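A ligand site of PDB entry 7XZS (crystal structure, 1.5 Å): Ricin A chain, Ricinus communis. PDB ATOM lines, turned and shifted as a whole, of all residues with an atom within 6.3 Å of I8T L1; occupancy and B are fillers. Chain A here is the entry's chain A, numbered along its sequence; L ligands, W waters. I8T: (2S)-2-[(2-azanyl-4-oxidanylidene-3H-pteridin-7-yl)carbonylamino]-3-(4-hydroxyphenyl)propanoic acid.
O of Gly 128 is in hydrogen-bond range of N2 of I8T L1, 3.1 Å away.
ND2 of Asn 85 lies within hydrogen-bond range of N1 of I8T L2.
The backbone NH (N) of Tyr 130 lies within hydrogen-bond range of an oxygen (OAQ) of I8T L1.
The guanidinium group (NH2) of Arg 187 sits at hydrogen-bond distance from an oxygen (O4) of I8T L1 (2.8 Å).
O of Val 88 lies within hydrogen-bond range of N2 of I8T L1.
Water W1 lies within hydrogen-bond range of an oxygen (OAQ) of I8T L1 (2.9 Å), the side-chain carboxylate (OD2) of Asp 131 (3.0 Å) and the backbone NH (N) of Tyr 130 (3.5 Å).
N of Phe 100 lies within hydrogen-bond range of O of Val 89, 3.1 Å away.
The guanidinium group of Arg 187 lies within salt-bridge range of the side-chain carboxylate of Glu 184, at 3.1 Å.
NH2 of Arg 187 is in hydrogen-bond range of O of Asn 85, 2.7 Å away.
O of Ile 179 sits at hydrogen-bond distance from N of Glu 184, 3.0 Å away.
The guanidinium group (NH1) of Arg 141 lies within hydrogen-bond range of the side-chain amide oxygen (OD1) of Asn 216, 2.9 Å away.
OE2 of Glu 184 sits at hydrogen-bond distance from OH of Tyr 130.
OH of Tyr 87 lies close to N of Gly 128 (3.4 Å).
The guanidinium group (NH1) of Arg 141 is in salt-bridge range of the side-chain carboxylate (OE1) of Glu 215.
A nitrogen (N) of I8T L1 sits at hydrogen-bond distance from an oxygen (OH) of I8T L2, at 3.2 Å.
Residues that only touch I8T L1: Asn 216 (3.2 Å), Tyr 87 (3.2 Å), Ile 179 (3.4 Å), Ser 183 (3.5 Å), Ala 86 (3.5 Å), Asn 129 (3.5 Å), Phe 100 (3.6 Å), Arg 141 (3.8 Å), Glu 184 (3.8 Å) and Glu 215 (3.99 Å).
Hydrophobic or aromatic side chains within 4 Å of I8T L1: Tyr 87, Val 88, Phe 100, Tyr 130 and Ile 179.
Of the 19 residues printed, 14 come within 4 Å of I8T L1.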
ATOM      1  N   ASN A  85     -31.657  -6.985  -5.578  1.00  0.00           N
ATOM      2  CA  ASN A  85     -30.432  -6.564  -6.277  1.00  0.00           C
ATOM      3  C   ASN A  85     -30.505  -6.622  -7.803  1.00  0.00           C
ATOM      4  O   ASN A  85     -29.510  -6.324  -8.467  1.00  0.00           O
ATOM      5  CB  ASN A  85     -29.220  -7.352  -5.759  1.00  0.00           C
ATOM      6  CG  ASN A  85     -29.418  -8.857  -5.856  1.00  0.00           C
ATOM      7  OD1 ASN A  85     -30.345  -9.346  -6.522  1.00  0.00           O
ATOM      8  ND2 ASN A  85     -28.555  -9.609  -5.179  1.00  0.00           N
ATOM      9  N   ALA A  86     -31.672  -6.998  -8.333  1.00  0.00           N
ATOM     10  CA  ALA A  86     -31.904  -7.232  -9.775  1.00  0.00           C
ATOM     11  C   ALA A  86     -31.054  -8.355 -10.388  1.00  0.00           C
ATOM     12  O   ALA A  86     -30.961  -8.496 -11.602  1.00  0.00           O
ATOM     13  CB  ALA A  86     -31.790  -5.924 -10.572  1.00  0.00           C
ATOM     14  N   TYR A  87     -30.460  -9.190  -9.530  1.00  0.00           N
ATOM     15  CA  TYR A  87     -29.577 -10.294  -9.939  1.00  0.00           C
ATOM     16  C   TYR A  87     -30.381 -11.376 -10.662  1.00  0.00           C
ATOM     17  O   TYR A  87     -31.453 -11.778 -10.197  1.00  0.00           O
ATOM     18  CB  TYR A  87     -28.931 -10.876  -8.689  1.00  0.00           C
ATOM     19  CG  TYR A  87     -27.701 -11.709  -8.873  1.00  0.00           C
ATOM     20  CD1 TYR A  87     -26.432 -11.124  -8.826  1.00  0.00           C
ATOM     21  CD2 TYR A  87     -27.796 -13.089  -9.050  1.00  0.00           C
ATOM     22  CE1 TYR A  87     -25.288 -11.904  -8.971  1.00  0.00           C
ATOM     23  CE2 TYR A  87     -26.665 -13.879  -9.221  1.00  0.00           C
ATOM     24  CZ  TYR A  87     -25.415 -13.272  -9.177  1.00  0.00           C
ATOM     25  OH  TYR A  87     -24.302 -14.058  -9.325  1.00  0.00           O
ATOM     26  N   VAL A  88     -29.872 -11.804 -11.816  1.00  0.00           N
ATOM     27  CA  VAL A  88     -30.430 -12.963 -12.523  1.00  0.00           C
ATOM     28  C   VAL A  88     -29.959 -14.213 -11.779  1.00  0.00           C
ATOM     29  O   VAL A  88     -28.769 -14.523 -11.772  1.00  0.00           O
ATOM     30  CB  VAL A  88     -29.972 -13.002 -14.006  1.00  0.00           C
ATOM     31  CG1 VAL A  88     -30.528 -14.230 -14.718  1.00  0.00           C
ATOM     32  CG2 VAL A  88     -30.404 -11.734 -14.744  1.00  0.00           C
ATOM     33  N   VAL A  89     -30.892 -14.910 -11.136  1.00  0.00           N
ATOM     34  CA  VAL A  89     -30.553 -16.066 -10.285  1.00  0.00           C
ATOM     35  C   VAL A  89     -30.616 -17.393 -11.030  1.00  0.00           C
ATOM     36  O   VAL A  89     -30.053 -18.400 -10.586  1.00  0.00           O
ATOM     37  CB  VAL A  89     -31.383 -16.133  -8.970  1.00  0.00           C
ATOM     38  CG1 VAL A  89     -31.182 -14.871  -8.135  1.00  0.00           C
ATOM     39  CG2 VAL A  89     -32.864 -16.370  -9.247  1.00  0.00           C
ATOM     40  N   PHE A 100     -27.842 -20.494 -10.797  1.00  0.00           N
ATOM     41  CA  PHE A 100     -26.451 -20.277 -10.410  1.00  0.00           C
ATOM     42  C   PHE A 100     -26.221 -20.777  -8.984  1.00  0.00           C
ATOM     43  O   PHE A 100     -27.160 -20.789  -8.179  1.00  0.00           O
ATOM     44  CB  PHE A 100     -26.077 -18.799 -10.508  1.00  0.00           C
ATOM     45  CG  PHE A 100     -26.122 -18.260 -11.912  1.00  0.00           C
ATOM     46  CD1 PHE A 100     -25.266 -18.755 -12.901  1.00  0.00           C
ATOM     47  CD2 PHE A 100     -27.012 -17.241 -12.244  1.00  0.00           C
ATOM     48  CE1 PHE A 100     -25.299 -18.249 -14.195  1.00  0.00           C
ATOM     49  CE2 PHE A 100     -27.058 -16.734 -13.544  1.00  0.00           C
ATOM     50  CZ  PHE A 100     -26.199 -17.234 -14.525  1.00  0.00           C
ATOM     51  N   GLY A 128     -22.868 -16.933 -10.464  1.00  0.00           N
ATOM     52  CA  GLY A 128     -23.286 -16.145 -11.615  1.00  0.00           C
ATOM     53  C   GLY A 128     -22.710 -14.743 -11.750  1.00  0.00           C
ATOM     54  O   GLY A 128     -23.206 -13.976 -12.565  1.00  0.00           O
ATOM     55  N   ASN A 129     -21.690 -14.414 -10.958  1.00  0.00           N
ATOM     56  CA  ASN A 129     -21.017 -13.116 -11.069  1.00  0.00           C
ATOM     57  C   ASN A 129     -20.207 -13.014 -12.369  1.00  0.00           C
ATOM     58  O   ASN A 129     -19.840 -14.034 -12.951  1.00  0.00           O
ATOM     59  CB  ASN A 129     -20.101 -12.848  -9.868  1.00  0.00           C
ATOM     60  CG  ASN A 129     -20.855 -12.677  -8.557  1.00  0.00           C
ATOM     61  OD1 ASN A 129     -22.077 -12.559  -8.527  1.00  0.00           O
ATOM     62  ND2 ASN A 129     -20.100 -12.653  -7.467  1.00  0.00           N
ATOM     63  N   TYR A 130     -19.956 -11.776 -12.810  1.00  0.00           N
ATOM     64  CA  TYR A 130     -19.207 -11.530 -14.052  1.00  0.00           C
ATOM     65  C   TYR A 130     -17.859 -12.243 -14.082  1.00  0.00           C
ATOM     66  O   TYR A 130     -17.520 -12.849 -15.098  1.00  0.00           O
ATOM     67  CB  TYR A 130     -18.990 -10.032 -14.307  1.00  0.00           C
ATOM     68  CG  TYR A 130     -20.223  -9.251 -14.674  1.00  0.00           C
ATOM     69  CD1 TYR A 130     -21.160  -9.739 -15.603  1.00  0.00           C
ATOM     70  CD2 TYR A 130     -20.445  -7.985 -14.119  1.00  0.00           C
ATOM     71  CE1 TYR A 130     -22.287  -8.994 -15.935  1.00  0.00           C
ATOM     72  CE2 TYR A 130     -21.570  -7.245 -14.443  1.00  0.00           C
ATOM     73  CZ  TYR A 130     -22.485  -7.751 -15.354  1.00  0.00           C
ATOM     74  OH  TYR A 130     -23.586  -7.017 -15.679  1.00  0.00           O
ATOM     75  N   ASP A 131     -17.103 -12.183 -12.972  1.00  0.00           N
ATOM     76  CA  ASP A 131     -15.781 -12.820 -12.886  1.00  0.00           C
ATOM     77  C   ASP A 131     -15.789 -14.282 -13.316  1.00  0.00           C
ATOM     78  O   ASP A 131     -14.973 -14.696 -14.145  1.00  0.00           O
ATOM     79  CB  ASP A 131     -15.121 -12.637 -11.498  1.00  0.00           C
ATOM     80  CG  ASP A 131     -16.060 -12.965 -10.325  1.00  0.00           C
ATOM     81  OD1 ASP A 131     -16.900 -13.888 -10.395  1.00  0.00           O
ATOM     82  OD2 ASP A 131     -15.938 -12.280  -9.288  1.00  0.00           O
ATOM     83  N   LEU A 133     -18.372 -15.859 -14.930  1.00  0.00           N
ATOM     84  CA  LEU A 133     -18.971 -15.996 -16.256  1.00  0.00           C
ATOM     85  C   LEU A 133     -17.986 -15.646 -17.374  1.00  0.00           C
ATOM     86  O   LEU A 133     -17.967 -16.328 -18.403  1.00  0.00           O
ATOM     87  CB  LEU A 133     -20.267 -15.181 -16.383  1.00  0.00           C
ATOM     88  CG  LEU A 133     -21.479 -15.619 -15.542  1.00  0.00           C
ATOM     89  CD1 LEU A 133     -22.635 -14.672 -15.821  1.00  0.00           C
ATOM     90  CD2 LEU A 133     -21.912 -17.067 -15.806  1.00  0.00           C
ATOM     91  N   ARG A 141     -16.186  -8.836 -20.478  1.00  0.00           N
ATOM     92  CA  ARG A 141     -17.314  -7.997 -20.915  1.00  0.00           C
ATOM     93  C   ARG A 141     -16.917  -7.014 -22.010  1.00  0.00           C
ATOM     94  O   ARG A 141     -17.676  -6.832 -22.969  1.00  0.00           O
ATOM     95  CB  ARG A 141     -17.912  -7.242 -19.734  1.00  0.00           C
ATOM     96  CG  ARG A 141     -18.883  -8.048 -18.882  1.00  0.00           C
ATOM     97  CD  ARG A 141     -19.200  -7.277 -17.609  1.00  0.00           C
ATOM     98  NE  ARG A 141     -18.097  -7.327 -16.639  1.00  0.00           N
ATOM     99  CZ  ARG A 141     -17.880  -6.436 -15.681  1.00  0.00           C
ATOM    100  NH1 ARG A 141     -18.673  -5.369 -15.536  1.00  0.00           N
ATOM    101  NH2 ARG A 141     -16.853  -6.593 -14.852  1.00  0.00           N
ATOM    102  N   ILE A 179     -27.741 -10.324 -18.702  1.00  0.00           N
ATOM    103  CA  ILE A 179     -27.557  -9.578 -17.460  1.00  0.00           C
ATOM    104  C   ILE A 179     -27.385  -8.088 -17.738  1.00  0.00           C
ATOM    105  O   ILE A 179     -28.009  -7.246 -17.083  1.00  0.00           O
ATOM    106  CB  ILE A 179     -26.383 -10.151 -16.634  1.00  0.00           C
ATOM    107  CG1 ILE A 179     -26.724 -11.533 -16.081  1.00  0.00           C
ATOM    108  CG2 ILE A 179     -26.008  -9.211 -15.492  1.00  0.00           C
ATOM    109  CD1 ILE A 179     -25.502 -12.368 -15.765  1.00  0.00           C
ATOM    110  N   SER A 183     -30.684  -6.446 -16.402  1.00  0.00           N
ATOM    111  CA  SER A 183     -30.390  -5.981 -15.048  1.00  0.00           C
ATOM    112  C   SER A 183     -29.599  -4.687 -15.002  1.00  0.00           C
ATOM    113  O   SER A 183     -29.982  -3.760 -14.284  1.00  0.00           O
ATOM    114  CB  SER A 183     -29.673  -7.077 -14.253  1.00  0.00           C
ATOM    115  OG  SER A 183     -30.465  -8.241 -14.237  1.00  0.00           O
ATOM    116  N   GLU A 184     -28.512  -4.584 -15.765  1.00  0.00           N
ATOM    117  CA  GLU A 184     -27.714  -3.355 -15.747  1.00  0.00           C
ATOM    118  C   GLU A 184     -28.466  -2.165 -16.328  1.00  0.00           C
ATOM    119  O   GLU A 184     -28.344  -1.045 -15.823  1.00  0.00           O
ATOM    120  CB  GLU A 184     -26.345  -3.519 -16.434  1.00  0.00           C
ATOM    121  CG  GLU A 184     -25.469  -4.594 -15.837  1.00  0.00           C
ATOM    122  CD  GLU A 184     -24.887  -4.289 -14.457  1.00  0.00           C
ATOM    123  OE1 GLU A 184     -25.290  -3.304 -13.796  1.00  0.00           O
ATOM    124  OE2 GLU A 184     -24.008  -5.063 -14.018  1.00  0.00           O
ATOM    125  N   ARG A 187     -30.790  -0.971 -13.687  1.00  0.00           N
ATOM    126  CA  ARG A 187     -30.039  -0.239 -12.655  1.00  0.00           C
ATOM    127  C   ARG A 187     -29.608   1.163 -13.098  1.00  0.00           C
ATOM    128  O   ARG A 187     -29.615   2.092 -12.273  1.00  0.00           O
ATOM    129  CB  ARG A 187     -28.785  -1.028 -12.251  1.00  0.00           C
ATOM    130  CG  ARG A 187     -29.065  -2.307 -11.481  1.00  0.00           C
ATOM    131  CD  ARG A 187     -27.802  -3.147 -11.403  1.00  0.00           C
ATOM    132  NE  ARG A 187     -28.078  -4.449 -10.818  1.00  0.00           N
ATOM    133  CZ  ARG A 187     -27.526  -5.591 -11.226  1.00  0.00           C
ATOM    134  NH1 ARG A 187     -26.684  -5.612 -12.255  1.00  0.00           N
ATOM    135  NH2 ARG A 187     -27.846  -6.726 -10.614  1.00  0.00           N
ATOM    136  N   GLU A 215     -21.139  -0.496 -14.174  1.00  0.00           N
ATOM    137  CA  GLU A 215     -21.497  -1.840 -13.702  1.00  0.00           C
ATOM    138  C   GLU A 215     -20.676  -2.233 -12.475  1.00  0.00           C
ATOM    139  O   GLU A 215     -21.232  -2.694 -11.469  1.00  0.00           O
ATOM    140  CB  GLU A 215     -21.286  -2.886 -14.797  1.00  0.00           C
ATOM    141  CG  GLU A 215     -22.171  -2.680 -16.021  1.00  0.00           C
ATOM    142  CD  GLU A 215     -21.860  -3.631 -17.151  1.00  0.00           C
ATOM    143  OE1 GLU A 215     -20.847  -4.378 -17.078  1.00  0.00           O
ATOM    144  OE2 GLU A 215     -22.614  -3.634 -18.143  1.00  0.00           O
ATOM    145  N   ASN A 216     -19.367  -2.009 -12.551  1.00  0.00           N
ATOM    146  CA  ASN A 216     -18.459  -2.361 -11.469  1.00  0.00           C
ATOM    147  C   ASN A 216     -18.658  -1.530 -10.209  1.00  0.00           C
ATOM    148  O   ASN A 216     -18.329  -2.008  -9.114  1.00  0.00           O
ATOM    149  CB  ASN A 216     -17.001  -2.253 -11.927  1.00  0.00           C
ATOM    150  CG  ASN A 216     -16.637  -3.304 -12.963  1.00  0.00           C
ATOM    151  OD1 ASN A 216     -17.379  -4.264 -13.204  1.00  0.00           O
ATOM    152  ND2 ASN A 216     -15.485  -3.121 -13.585  1.00  0.00           N
ATOM    153  N   SER A 217     -19.191  -0.322 -10.355  1.00  0.00           N
ATOM    154  CA  SER A 217     -19.326   0.610  -9.246  1.00  0.00           C
ATOM    155  C   SER A 217     -20.720   0.709  -8.635  1.00  0.00           C
ATOM    156  O   SER A 217     -20.929   1.519  -7.736  1.00  0.00           O
ATOM    157  CB  SER A 217     -18.857   2.011  -9.656  1.00  0.00           C
ATOM    158  OG  SER A 217     -17.532   1.988 -10.148  1.00  0.00           O
HETATM  159  C2  I8T L   1     -25.972 -12.121 -12.367  1.00  0.00           C
HETATM  160  C4  I8T L   1     -26.657  -9.808 -12.225  1.00  0.00           C
HETATM  161  C6  I8T L   1     -23.591  -7.875 -11.464  1.00  0.00           C
HETATM  162  C7  I8T L   1     -22.645  -8.901 -11.415  1.00  0.00           C
HETATM  163  N   I8T L   1     -20.987  -7.529 -10.488  1.00  0.00           N
HETATM  164  C   I8T L   1     -19.463  -7.669  -8.519  1.00  0.00           C
HETATM  165  O   I8T L   1     -18.511  -8.421  -8.218  1.00  0.00           O
HETATM  166  N1  I8T L   1     -24.694 -11.753 -12.117  1.00  0.00           N
HETATM  167  N2  I8T L   1     -26.258 -13.404 -12.571  1.00  0.00           N
HETATM  168  N3  I8T L   1     -26.977 -11.154 -12.439  1.00  0.00           N
HETATM  169  CD1 I8T L   1     -16.981  -4.991  -9.233  1.00  0.00           C
HETATM  170  CE1 I8T L   1     -15.583  -4.929  -9.145  1.00  0.00           C
HETATM  171  CZ  I8T L   1     -14.791  -5.697 -10.020  1.00  0.00           C
HETATM  172  OH  I8T L   1     -13.436  -5.635  -9.927  1.00  0.00           O
HETATM  173  CE2 I8T L   1     -15.399  -6.519 -10.978  1.00  0.00           C
HETATM  174  CD2 I8T L   1     -16.790  -6.569 -11.063  1.00  0.00           C
HETATM  175  CG  I8T L   1     -17.580  -5.810 -10.193  1.00  0.00           C
HETATM  176  CB  I8T L   1     -19.122  -5.858 -10.277  1.00  0.00           C
HETATM  177  CA  I8T L   1     -19.608  -7.290 -10.011  1.00  0.00           C
HETATM  178  OXT I8T L   1     -20.309  -7.210  -7.713  1.00  0.00           O
HETATM  179  CAL I8T L   1     -21.300  -8.686 -11.097  1.00  0.00           C
HETATM  180  OAQ I8T L   1     -20.493  -9.612 -11.191  1.00  0.00           O
HETATM  181  N8  I8T L   1     -23.067 -10.171 -11.631  1.00  0.00           N
HETATM  182  C8A I8T L   1     -24.356 -10.463 -11.906  1.00  0.00           C
HETATM  183  O4  I8T L   1     -27.558  -8.978 -12.294  1.00  0.00           O
HETATM  184  C4A I8T L   1     -25.318  -9.451 -11.957  1.00  0.00           C
HETATM  185  N5  I8T L   1     -24.941  -8.177 -11.745  1.00  0.00           N
HETATM  186  C2  I8T L   2     -28.681 -13.579  -5.360  1.00  0.00           C
HETATM  187  C4  I8T L   2     -26.636 -14.785  -5.863  1.00  0.00           C
HETATM  188  C6  I8T L   2     -23.891 -12.324  -5.624  1.00  0.00           C
HETATM  189  C7  I8T L   2     -24.627 -11.183  -5.277  1.00  0.00           C
HETATM  190  N   I8T L   2     -24.563  -9.193  -4.094  1.00  0.00           N
HETATM  191  C   I8T L   2     -23.956  -7.731  -2.149  1.00  0.00           C
HETATM  192  O   I8T L   2     -24.330  -8.700  -1.457  1.00  0.00           O
HETATM  193  N1  I8T L   2     -27.968 -12.450  -5.182  1.00  0.00           N
HETATM  194  N2  I8T L   2     -29.991 -13.567  -5.197  1.00  0.00           N
HETATM  195  N3  I8T L   2     -28.032 -14.778  -5.705  1.00  0.00           N
HETATM  196  CD1 I8T L   2     -23.382  -5.561  -5.756  1.00  0.00           C
HETATM  197  CE1 I8T L   2     -22.886  -5.217  -7.012  1.00  0.00           C
HETATM  198  CZ  I8T L   2     -23.498  -5.712  -8.172  1.00  0.00           C
HETATM  199  OH  I8T L   2     -22.984  -5.355  -9.367  1.00  0.00           O
HETATM  200  CE2 I8T L   2     -24.604  -6.558  -8.080  1.00  0.00           C
HETATM  201  CD2 I8T L   2     -25.106  -6.910  -6.814  1.00  0.00           C
HETATM  202  CG  I8T L   2     -24.488  -6.407  -5.665  1.00  0.00           C
HETATM  203  CB  I8T L   2     -25.002  -6.774  -4.269  1.00  0.00           C
HETATM  204  CA  I8T L   2     -24.073  -7.854  -3.684  1.00  0.00           C
HETATM  205  OXT I8T L   2     -23.444  -6.679  -1.704  1.00  0.00           O
HETATM  206  CAL I8T L   2     -23.987  -9.950  -5.060  1.00  0.00           C
HETATM  207  OAQ I8T L   2     -22.971  -9.627  -5.682  1.00  0.00           O
HETATM  208  N8  I8T L   2     -25.964 -11.266  -5.146  1.00  0.00           N
HETATM  209  C8A I8T L   2     -26.623 -12.429  -5.328  1.00  0.00           C
HETATM  210  O4  I8T L   2     -26.086 -15.836  -6.170  1.00  0.00           O
HETATM  211  C4A I8T L   2     -25.924 -13.595  -5.687  1.00  0.00           C
HETATM  212  N5  I8T L   2     -24.578 -13.541  -5.826  1.00  0.00           N
HETATM  213  O   HOH W   1     -17.725 -10.312 -10.609  1.00  0.00           O
